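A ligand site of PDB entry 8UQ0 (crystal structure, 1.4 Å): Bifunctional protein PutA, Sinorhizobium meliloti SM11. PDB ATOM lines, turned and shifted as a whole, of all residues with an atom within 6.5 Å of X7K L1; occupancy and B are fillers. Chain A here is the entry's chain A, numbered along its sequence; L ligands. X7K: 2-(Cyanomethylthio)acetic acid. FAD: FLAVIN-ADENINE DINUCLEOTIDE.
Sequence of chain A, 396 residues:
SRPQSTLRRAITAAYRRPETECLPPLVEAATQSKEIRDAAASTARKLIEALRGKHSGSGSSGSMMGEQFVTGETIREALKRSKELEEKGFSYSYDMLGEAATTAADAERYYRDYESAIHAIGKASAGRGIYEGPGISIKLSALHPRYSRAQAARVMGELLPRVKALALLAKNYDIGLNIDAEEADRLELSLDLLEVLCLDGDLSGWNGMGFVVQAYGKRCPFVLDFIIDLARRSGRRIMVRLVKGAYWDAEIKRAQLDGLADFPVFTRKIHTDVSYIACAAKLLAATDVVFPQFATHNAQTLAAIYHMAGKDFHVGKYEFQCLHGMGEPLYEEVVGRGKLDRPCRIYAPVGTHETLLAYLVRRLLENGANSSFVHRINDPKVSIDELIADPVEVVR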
ATOM      1  N   ASP A  95       5.774   8.234  13.908  1.00  0.00           N
ATOM      2  CA  ASP A  95       6.327   7.997  15.234  1.00  0.00           C
ATOM      3  C   ASP A  95       7.806   7.660  15.044  1.00  0.00           C
ATOM      4  O   ASP A  95       8.131   6.552  14.600  1.00  0.00           O
ATOM      5  CB  ASP A  95       5.587   6.827  15.880  1.00  0.00           C
ATOM      6  CG  ASP A  95       6.329   6.257  17.082  1.00  0.00           C
ATOM      7  OD1 ASP A  95       6.908   7.059  17.835  1.00  0.00           O
ATOM      8  OD2 ASP A  95       6.314   5.008  17.258  1.00  0.00           O
ATOM      9  N   LEU A  97      10.706   6.162  16.393  1.00  0.00           N
ATOM     10  CA  LEU A  97      10.767   5.188  17.471  1.00  0.00           C
ATOM     11  C   LEU A  97      11.839   5.563  18.480  1.00  0.00           C
ATOM     12  O   LEU A  97      12.868   6.151  18.141  1.00  0.00           O
ATOM     13  CB  LEU A  97      11.043   3.802  16.888  1.00  0.00           C
ATOM     14  CG  LEU A  97       9.850   3.152  16.181  1.00  0.00           C
ATOM     15  CD1 LEU A  97      10.309   2.146  15.137  1.00  0.00           C
ATOM     16  CD2 LEU A  97       8.897   2.499  17.201  1.00  0.00           C
ATOM     17  N   GLU A  99      12.121   5.476  23.197  1.00  0.00           N
ATOM     18  CA  GLU A  99      11.365   5.730  24.418  1.00  0.00           C
ATOM     19  C   GLU A  99      12.258   5.413  25.599  1.00  0.00           C
ATOM     20  O   GLU A  99      13.320   4.802  25.462  1.00  0.00           O
ATOM     21  CB  GLU A  99      10.092   4.880  24.466  1.00  0.00           C
ATOM     22  CG  GLU A  99      10.338   3.367  24.510  1.00  0.00           C
ATOM     23  CD  GLU A  99       9.046   2.608  24.379  1.00  0.00           C
ATOM     24  OE1 GLU A  99       8.355   2.789  23.361  1.00  0.00           O
ATOM     25  OE2 GLU A  99       8.715   1.844  25.300  1.00  0.00           O
ATOM     26  N   LYS A 139       6.735  10.612  22.401  1.00  0.00           N
ATOM     27  CA  LYS A 139       6.669  10.043  23.738  1.00  0.00           C
ATOM     28  C   LYS A 139       7.511  10.882  24.684  1.00  0.00           C
ATOM     29  O   LYS A 139       8.701  11.092  24.446  1.00  0.00           O
ATOM     30  CB  LYS A 139       7.180   8.589  23.749  1.00  0.00           C
ATOM     31  CG  LYS A 139       6.107   7.593  23.286  1.00  0.00           C
ATOM     32  CD  LYS A 139       6.659   6.173  23.257  1.00  0.00           C
ATOM     33  CE  LYS A 139       5.526   5.172  22.982  1.00  0.00           C
ATOM     34  NZ  LYS A 139       5.013   5.282  21.593  1.00  0.00           N
ATOM     35  N   ASP A 180       1.820  10.778  22.950  1.00  0.00           N
ATOM     36  CA  ASP A 180       1.380   9.419  23.259  1.00  0.00           C
ATOM     37  C   ASP A 180       1.217   9.227  24.771  1.00  0.00           C
ATOM     38  O   ASP A 180       1.910   9.838  25.584  1.00  0.00           O
ATOM     39  CB  ASP A 180       2.421   8.401  22.771  1.00  0.00           C
ATOM     40  CG  ASP A 180       2.406   8.193  21.252  1.00  0.00           C
ATOM     41  OD1 ASP A 180       1.522   8.723  20.531  1.00  0.00           O
ATOM     42  OD2 ASP A 180       3.330   7.482  20.772  1.00  0.00           O
ATOM     43  N   ALA A 181       0.297   8.329  25.152  1.00  0.00           N
ATOM     44  CA  ALA A 181       0.123   7.971  26.554  1.00  0.00           C
ATOM     45  C   ALA A 181       0.954   6.737  26.888  1.00  0.00           C
ATOM     46  O   ALA A 181       0.945   5.754  26.136  1.00  0.00           O
ATOM     47  CB  ALA A 181      -1.342   7.665  26.849  1.00  0.00           C
ATOM     48  N   GLU A 182       1.635   6.789  28.027  1.00  0.00           N
ATOM     49  CA  GLU A 182       2.490   5.679  28.429  1.00  0.00           C
ATOM     50  C   GLU A 182       1.991   5.055  29.737  1.00  0.00           C
ATOM     51  O   GLU A 182       0.817   4.688  29.815  1.00  0.00           O
ATOM     52  CB  GLU A 182       3.955   6.122  28.447  1.00  0.00           C
ATOM     53  CG  GLU A 182       4.433   6.611  27.056  1.00  0.00           C
ATOM     54  CD  GLU A 182       5.878   7.084  27.073  1.00  0.00           C
ATOM     55  OE1 GLU A 182       6.788   6.226  27.101  1.00  0.00           O
ATOM     56  OE2 GLU A 182       6.099   8.313  27.092  1.00  0.00           O
ATOM     57  N   VAL A 212      -3.380  11.593  23.987  1.00  0.00           N
ATOM     58  CA  VAL A 212      -4.003  10.277  24.055  1.00  0.00           C
ATOM     59  C   VAL A 212      -4.610  10.064  25.436  1.00  0.00           C
ATOM     60  O   VAL A 212      -3.992  10.415  26.450  1.00  0.00           O
ATOM     61  CB  VAL A 212      -2.959   9.187  23.777  1.00  0.00           C
ATOM     62  CG1 VAL A 212      -3.568   7.763  23.886  1.00  0.00           C
ATOM     63  CG2 VAL A 212      -2.297   9.396  22.436  1.00  0.00           C
ATOM     64  N   ARG A 241      -6.907  11.493  21.069  1.00  0.00           N
ATOM     65  CA  ARG A 241      -6.853  10.117  20.592  1.00  0.00           C
ATOM     66  C   ARG A 241      -7.347   9.205  21.693  1.00  0.00           C
ATOM     67  O   ARG A 241      -6.706   9.085  22.745  1.00  0.00           O
ATOM     68  CB  ARG A 241      -5.449   9.713  20.161  1.00  0.00           C
ATOM     69  CG  ARG A 241      -5.444   8.290  19.608  1.00  0.00           C
ATOM     70  CD  ARG A 241      -4.040   7.693  19.534  1.00  0.00           C
ATOM     71  NE  ARG A 241      -3.205   8.423  18.597  1.00  0.00           N
ATOM     72  CZ  ARG A 241      -1.888   8.501  18.677  1.00  0.00           C
ATOM     73  NH1 ARG A 241      -1.210   7.897  19.641  1.00  0.00           N
ATOM     74  NH2 ARG A 241      -1.225   9.212  17.752  1.00  0.00           N
ATOM     75  N   ALA A 246      -1.922   0.237  25.696  1.00  0.00           N
ATOM     76  CA  ALA A 246      -0.882  -0.677  25.208  1.00  0.00           C
ATOM     77  C   ALA A 246      -0.070  -1.372  26.303  1.00  0.00           C
ATOM     78  O   ALA A 246       0.723  -2.263  25.981  1.00  0.00           O
ATOM     79  CB  ALA A 246       0.110   0.054  24.291  1.00  0.00           C
ATOM     80  N   TYR A 247      -0.228  -0.983  27.570  1.00  0.00           N
ATOM     81  CA  TYR A 247       0.677  -1.376  28.647  1.00  0.00           C
ATOM     82  C   TYR A 247      -0.018  -2.246  29.700  1.00  0.00           C
ATOM     83  O   TYR A 247       0.420  -2.289  30.852  1.00  0.00           O
ATOM     84  CB  TYR A 247       1.309  -0.143  29.296  1.00  0.00           C
ATOM     85  CG  TYR A 247       2.034   0.768  28.319  1.00  0.00           C
ATOM     86  CD1 TYR A 247       1.323   1.680  27.566  1.00  0.00           C
ATOM     87  CD2 TYR A 247       3.415   0.744  28.187  1.00  0.00           C
ATOM     88  CE1 TYR A 247       1.958   2.514  26.661  1.00  0.00           C
ATOM     89  CE2 TYR A 247       4.062   1.603  27.293  1.00  0.00           C
ATOM     90  CZ  TYR A 247       3.324   2.468  26.541  1.00  0.00           C
ATOM     91  OH  TYR A 247       3.945   3.313  25.639  1.00  0.00           O
ATOM     92  N   LEU A 323      -2.979   1.301  13.613  1.00  0.00           N
ATOM     93  CA  LEU A 323      -1.533   1.103  13.567  1.00  0.00           C
ATOM     94  C   LEU A 323      -1.097   0.562  12.205  1.00  0.00           C
ATOM     95  O   LEU A 323      -1.737  -0.344  11.648  1.00  0.00           O
ATOM     96  CB  LEU A 323      -1.080   0.116  14.651  1.00  0.00           C
ATOM     97  CG  LEU A 323      -1.309   0.565  16.110  1.00  0.00           C
ATOM     98  CD1 LEU A 323      -0.755  -0.479  17.094  1.00  0.00           C
ATOM     99  CD2 LEU A 323      -0.698   1.926  16.392  1.00  0.00           C
ATOM    100  N   TYR A 347      -0.900   5.364  12.298  1.00  0.00           N
ATOM    101  CA  TYR A 347       0.242   5.580  13.173  1.00  0.00           C
ATOM    102  C   TYR A 347       1.398   4.797  12.570  1.00  0.00           C
ATOM    103  O   TYR A 347       1.336   3.560  12.442  1.00  0.00           O
ATOM    104  CB  TYR A 347      -0.114   5.069  14.569  1.00  0.00           C
ATOM    105  CG  TYR A 347       0.904   5.349  15.646  1.00  0.00           C
ATOM    106  CD1 TYR A 347       1.968   4.503  15.846  1.00  0.00           C
ATOM    107  CD2 TYR A 347       0.796   6.470  16.474  1.00  0.00           C
ATOM    108  CE1 TYR A 347       2.914   4.744  16.835  1.00  0.00           C
ATOM    109  CE2 TYR A 347       1.717   6.724  17.473  1.00  0.00           C
ATOM    110  CZ  TYR A 347       2.776   5.861  17.635  1.00  0.00           C
ATOM    111  OH  TYR A 347       3.706   6.088  18.630  1.00  0.00           O
ATOM    112  N   ALA A 358      11.066  -2.382  21.698  1.00  0.00           N
ATOM    113  CA  ALA A 358      10.087  -2.188  22.764  1.00  0.00           C
ATOM    114  C   ALA A 358       8.667  -2.081  22.223  1.00  0.00           C
ATOM    115  O   ALA A 358       7.715  -2.611  22.809  1.00  0.00           O
ATOM    116  CB  ALA A 358      10.431  -0.936  23.574  1.00  0.00           C
ATOM    117  N   TYR A 359       8.509  -1.364  21.105  1.00  0.00           N
ATOM    118  CA  TYR A 359       7.218  -1.271  20.441  1.00  0.00           C
ATOM    119  C   TYR A 359       6.748  -2.648  19.977  1.00  0.00           C
ATOM    120  O   TYR A 359       5.570  -3.001  20.143  1.00  0.00           O
ATOM    121  CB  TYR A 359       7.379  -0.302  19.265  1.00  0.00           C
ATOM    122  CG  TYR A 359       6.151  -0.046  18.414  1.00  0.00           C
ATOM    123  CD1 TYR A 359       5.894  -0.813  17.284  1.00  0.00           C
ATOM    124  CD2 TYR A 359       5.272   0.986  18.718  1.00  0.00           C
ATOM    125  CE1 TYR A 359       4.788  -0.575  16.496  1.00  0.00           C
ATOM    126  CE2 TYR A 359       4.164   1.229  17.937  1.00  0.00           C
ATOM    127  CZ  TYR A 359       3.931   0.451  16.833  1.00  0.00           C
ATOM    128  OH  TYR A 359       2.805   0.754  16.069  1.00  0.00           O
ATOM    129  N   ARG A 362       5.072  -4.707  22.752  1.00  0.00           N
ATOM    130  CA  ARG A 362       3.682  -4.349  22.983  1.00  0.00           C
ATOM    131  C   ARG A 362       2.775  -4.849  21.862  1.00  0.00           C
ATOM    132  O   ARG A 362       1.630  -5.238  22.135  1.00  0.00           O
ATOM    133  CB  ARG A 362       3.544  -2.841  23.226  1.00  0.00           C
ATOM    134  CG  ARG A 362       4.202  -2.414  24.543  1.00  0.00           C
ATOM    135  CD  ARG A 362       3.938  -0.971  24.889  1.00  0.00           C
ATOM    136  NE  ARG A 362       4.510  -0.073  23.890  1.00  0.00           N
ATOM    137  CZ  ARG A 362       5.737   0.424  23.943  1.00  0.00           C
ATOM    138  NH1 ARG A 362       6.567   0.136  24.917  1.00  0.00           N
ATOM    139  NH2 ARG A 362       6.134   1.247  22.970  1.00  0.00           N
ATOM    140  N   ARG A 363       3.261  -4.883  20.615  1.00  0.00           N
ATOM    141  CA  ARG A 363       2.456  -5.439  19.530  1.00  0.00           C
ATOM    142  C   ARG A 363       2.283  -6.951  19.682  1.00  0.00           C
ATOM    143  O   ARG A 363       1.233  -7.485  19.321  1.00  0.00           O
ATOM    144  CB  ARG A 363       3.084  -5.126  18.170  1.00  0.00           C
ATOM    145  CG  ARG A 363       3.274  -3.604  17.854  1.00  0.00           C
ATOM    146  CD  ARG A 363       1.977  -2.819  17.620  1.00  0.00           C
ATOM    147  NE  ARG A 363       1.234  -2.569  18.847  1.00  0.00           N
ATOM    148  CZ  ARG A 363       1.604  -1.697  19.779  1.00  0.00           C
ATOM    149  NH1 ARG A 363       2.748  -1.038  19.688  1.00  0.00           N
ATOM    150  NH2 ARG A 363       0.789  -1.459  20.800  1.00  0.00           N
ATOM    151  N   GLU A 366      -0.385  -7.461  22.227  1.00  0.00           N
ATOM    152  CA  GLU A 366      -1.676  -7.099  21.660  1.00  0.00           C
ATOM    153  C   GLU A 366      -2.172  -8.170  20.691  1.00  0.00           C
ATOM    154  O   GLU A 366      -3.320  -8.619  20.770  1.00  0.00           O
ATOM    155  CB  GLU A 366      -1.542  -5.738  20.972  1.00  0.00           C
ATOM    156  CG  GLU A 366      -2.765  -5.264  20.217  1.00  0.00           C
ATOM    157  CD  GLU A 366      -2.533  -3.914  19.559  1.00  0.00           C
ATOM    158  OE1 GLU A 366      -1.383  -3.401  19.596  1.00  0.00           O
ATOM    159  OE2 GLU A 366      -3.494  -3.335  19.034  1.00  0.00           O
HETATM  160  C01 X7K L   1       1.371   4.207  20.199  1.00  0.00           C
HETATM  161  C02 X7K L   1       0.705   2.888  20.011  1.00  0.00           C
HETATM  162  C05 X7K L   1       2.066   2.841  22.789  1.00  0.00           C
HETATM  163  C06 X7K L   1       3.058   1.973  21.924  1.00  0.00           C
HETATM  164  N03 X7K L   1       0.121   1.910  19.826  1.00  0.00           N
HETATM  165  O07 X7K L   1       4.013   2.560  21.360  1.00  0.00           O
HETATM  166  O08 X7K L   1       2.808   0.770  21.832  1.00  0.00           O
HETATM  167  S04 X7K L   1       1.836   4.457  21.957  1.00  0.00           S
HETATM  168  PA  FAD L   2      -9.368  -4.919  21.293  1.00  0.00           P
HETATM  169  O1A FAD L   2      -8.991  -6.319  21.040  1.00  0.00           O
HETATM  170  O2A FAD L   2     -10.855  -4.592  21.253  1.00  0.00           O
HETATM  171  O5B FAD L   2      -8.895  -4.468  22.666  1.00  0.00           O
HETATM  172  C5B FAD L   2      -7.643  -4.939  23.227  1.00  0.00           C
HETATM  173  C4B FAD L   2      -7.270  -4.075  24.401  1.00  0.00           C
HETATM  174  O4B FAD L   2      -8.094  -4.370  25.545  1.00  0.00           O
HETATM  175  C3B FAD L   2      -5.851  -4.245  24.911  1.00  0.00           C
HETATM  176  O3B FAD L   2      -4.952  -3.550  24.037  1.00  0.00           O
HETATM  177  C2B FAD L   2      -5.966  -3.655  26.320  1.00  0.00           C
HETATM  178  O2B FAD L   2      -5.995  -2.232  26.323  1.00  0.00           O
HETATM  179  C1B FAD L   2      -7.360  -4.116  26.739  1.00  0.00           C
HETATM  180  N9A FAD L   2      -7.396  -5.321  27.573  1.00  0.00           N
HETATM  181  C8A FAD L   2      -7.020  -6.586  27.225  1.00  0.00           C
HETATM  182  N7A FAD L   2      -7.185  -7.477  28.184  1.00  0.00           N
HETATM  183  C5A FAD L   2      -7.738  -6.739  29.222  1.00  0.00           C
HETATM  184  C6A FAD L   2      -8.163  -7.097  30.508  1.00  0.00           C
HETATM  185  N6A FAD L   2      -8.104  -8.343  30.995  1.00  0.00           N
HETATM  186  N1A FAD L   2      -8.677  -6.120  31.300  1.00  0.00           N
HETATM  187  C2A FAD L   2      -8.746  -4.877  30.813  1.00  0.00           C
HETATM  188  N3A FAD L   2      -8.379  -4.432  29.615  1.00  0.00           N
HETATM  189  C4A FAD L   2      -7.875  -5.411  28.858  1.00  0.00           C
HETATM  190  N1  FAD L   2      -2.166   2.774  23.648  1.00  0.00           N
HETATM  191  C2  FAD L   2      -1.503   3.481  24.597  1.00  0.00           C
HETATM  192  O2  FAD L   2      -1.402   3.047  25.752  1.00  0.00           O
HETATM  193  N3  FAD L   2      -0.911   4.694  24.273  1.00  0.00           N
HETATM  194  C4  FAD L   2      -0.932   5.304  23.025  1.00  0.00           C
HETATM  195  O4  FAD L   2      -0.419   6.404  22.874  1.00  0.00           O
HETATM  196  C4X FAD L   2      -1.649   4.537  22.019  1.00  0.00           C
HETATM  197  N5  FAD L   2      -1.727   5.029  20.779  1.00  0.00           N
HETATM  198  C5X FAD L   2      -2.431   4.287  19.833  1.00  0.00           C
HETATM  199  C6  FAD L   2      -2.527   4.770  18.520  1.00  0.00           C
HETATM  200  C7  FAD L   2      -3.234   4.069  17.545  1.00  0.00           C
HETATM  201  C7M FAD L   2      -3.334   4.632  16.151  1.00  0.00           C
HETATM  202  C8  FAD L   2      -3.832   2.845  17.876  1.00  0.00           C
HETATM  203  C8M FAD L   2      -4.603   2.049  16.854  1.00  0.00           C
HETATM  204  C9  FAD L   2      -3.732   2.350  19.172  1.00  0.00           C
HETATM  205  C9A FAD L   2      -3.028   3.059  20.141  1.00  0.00           C
HETATM  206  N10 FAD L   2      -2.895   2.558  21.449  1.00  0.00           N
HETATM  207  C10 FAD L   2      -2.240   3.289  22.417  1.00  0.00           C
HETATM  208  C1' FAD L   2      -3.640   1.370  21.871  1.00  0.00           C
HETATM  209  C2' FAD L   2      -2.879   0.053  21.890  1.00  0.00           C
HETATM  210  O2' FAD L   2      -1.619   0.136  21.236  1.00  0.00           O
HETATM  211  C3' FAD L   2      -3.742  -1.013  21.198  1.00  0.00           C
HETATM  212  O3' FAD L   2      -3.654  -0.816  19.791  1.00  0.00           O
HETATM  213  C4' FAD L   2      -5.223  -1.031  21.586  1.00  0.00           C
HETATM  214  O4' FAD L   2      -5.357  -0.983  23.010  1.00  0.00           O
HETATM  215  C5' FAD L   2      -5.967  -2.210  20.986  1.00  0.00           C
HETATM  216  O5' FAD L   2      -7.387  -1.960  21.089  1.00  0.00           O
HETATM  217  P   FAD L   2      -8.380  -2.420  19.970  1.00  0.00           P
HETATM  218  O1P FAD L   2      -9.684  -1.672  20.232  1.00  0.00           O
HETATM  219  O2P FAD L   2      -7.759  -2.347  18.690  1.00  0.00           O
HETATM  220  O3P FAD L   2      -8.604  -3.967  20.284  1.00  0.00           O
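The guanidinium group (NE) of Arg 362 lies within salt-bridge range of an oxygen (O08) of X7K L1 (2.8 Å).
An oxygen (O08) of X7K L1 lies within salt-bridge range of the guanidinium group of Arg 363, at 2.8 Å.
The side-chain amino group (NZ) of Lys 139 lies within salt-bridge range of an oxygen (O07) of X7K L1 (2.9 Å).
The guanidinium group of Arg 363 is in hydrogen-bond range of an oxygen (O2') of FAD L2, 2.9 Å away.
An oxygen (O2) of FAD L2 sits at hydrogen-bond distance from the backbone NH of Ala 246 (2.9 Å).
An oxygen (O4) of FAD L2 is in hydrogen-bond range of the backbone NH (N) of Ala 181 (3.1 Å).
N3 of FAD L2 is in hydrogen-bond range of O of Ala 181, at 2.8 Å.
The guanidinium group (NH1) of Arg 241 is in hydrogen-bond range of a nitrogen (N5) of FAD L2 (3.1 Å).
O3' of FAD L2 lies within hydrogen-bond range of OE2 of Glu 366, at 2.6 Å.
The guanidinium group of Arg 362 is in salt-bridge range of the side-chain carboxylate of Glu 99 (2.7 Å).
O of Tyr 359 lies close to NH1 of Arg 363.
NE of Arg 363 lies within salt-bridge range of OE1 of Glu 366, at 2.8 Å.
NZ of Lys 139 is in hydrogen-bond range of OH of Tyr 347.
The side-chain amino group (NZ) of Lys 139 is in salt-bridge range of the side-chain carboxylate (OD2) of Asp 180 (2.9 Å).
The side-chain hydroxyl (OH) of Tyr 347 sits at hydrogen-bond distance from the side-chain carboxylate (OD2) of Asp 180 (2.6 Å).
The side-chain hydroxyl (OH) of Tyr 347 sits close to the side-chain carboxylate (OD2) of Asp 95 (3.1 Å).
The side-chain carboxylate of Asp 180 is in salt-bridge range of the guanidinium group of Arg 241, at 3.0 Å.
A sulfur (S04) of X7K L1 sits close to the side-chain carboxylate (OD2) of Asp 180.
Ala 246 touches X7K L1 (CB to O08, 3.7 Å).
Tyr 247 touches X7K L1 (OH to C05, 3.4 Å).
CD2 of Leu 323 touches N03 of X7K L1, at 3.5 Å.
Tyr 347 touches X7K L1.
Tyr 359 touches X7K L1 (CD2 to O07, 3.3 Å).
Hydrophobic or aromatic side chains within 4 Å of X7K L1: Ala 246, Tyr 247, Leu 323, Tyr 347 and Tyr 359.
The nearest printed residue that does not touch X7K L1 is Ala 181 (4.5 Å).
N03 of X7K L1 sits at hydrogen-bond distance from O2' of FAD L2 (2.9 Å).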
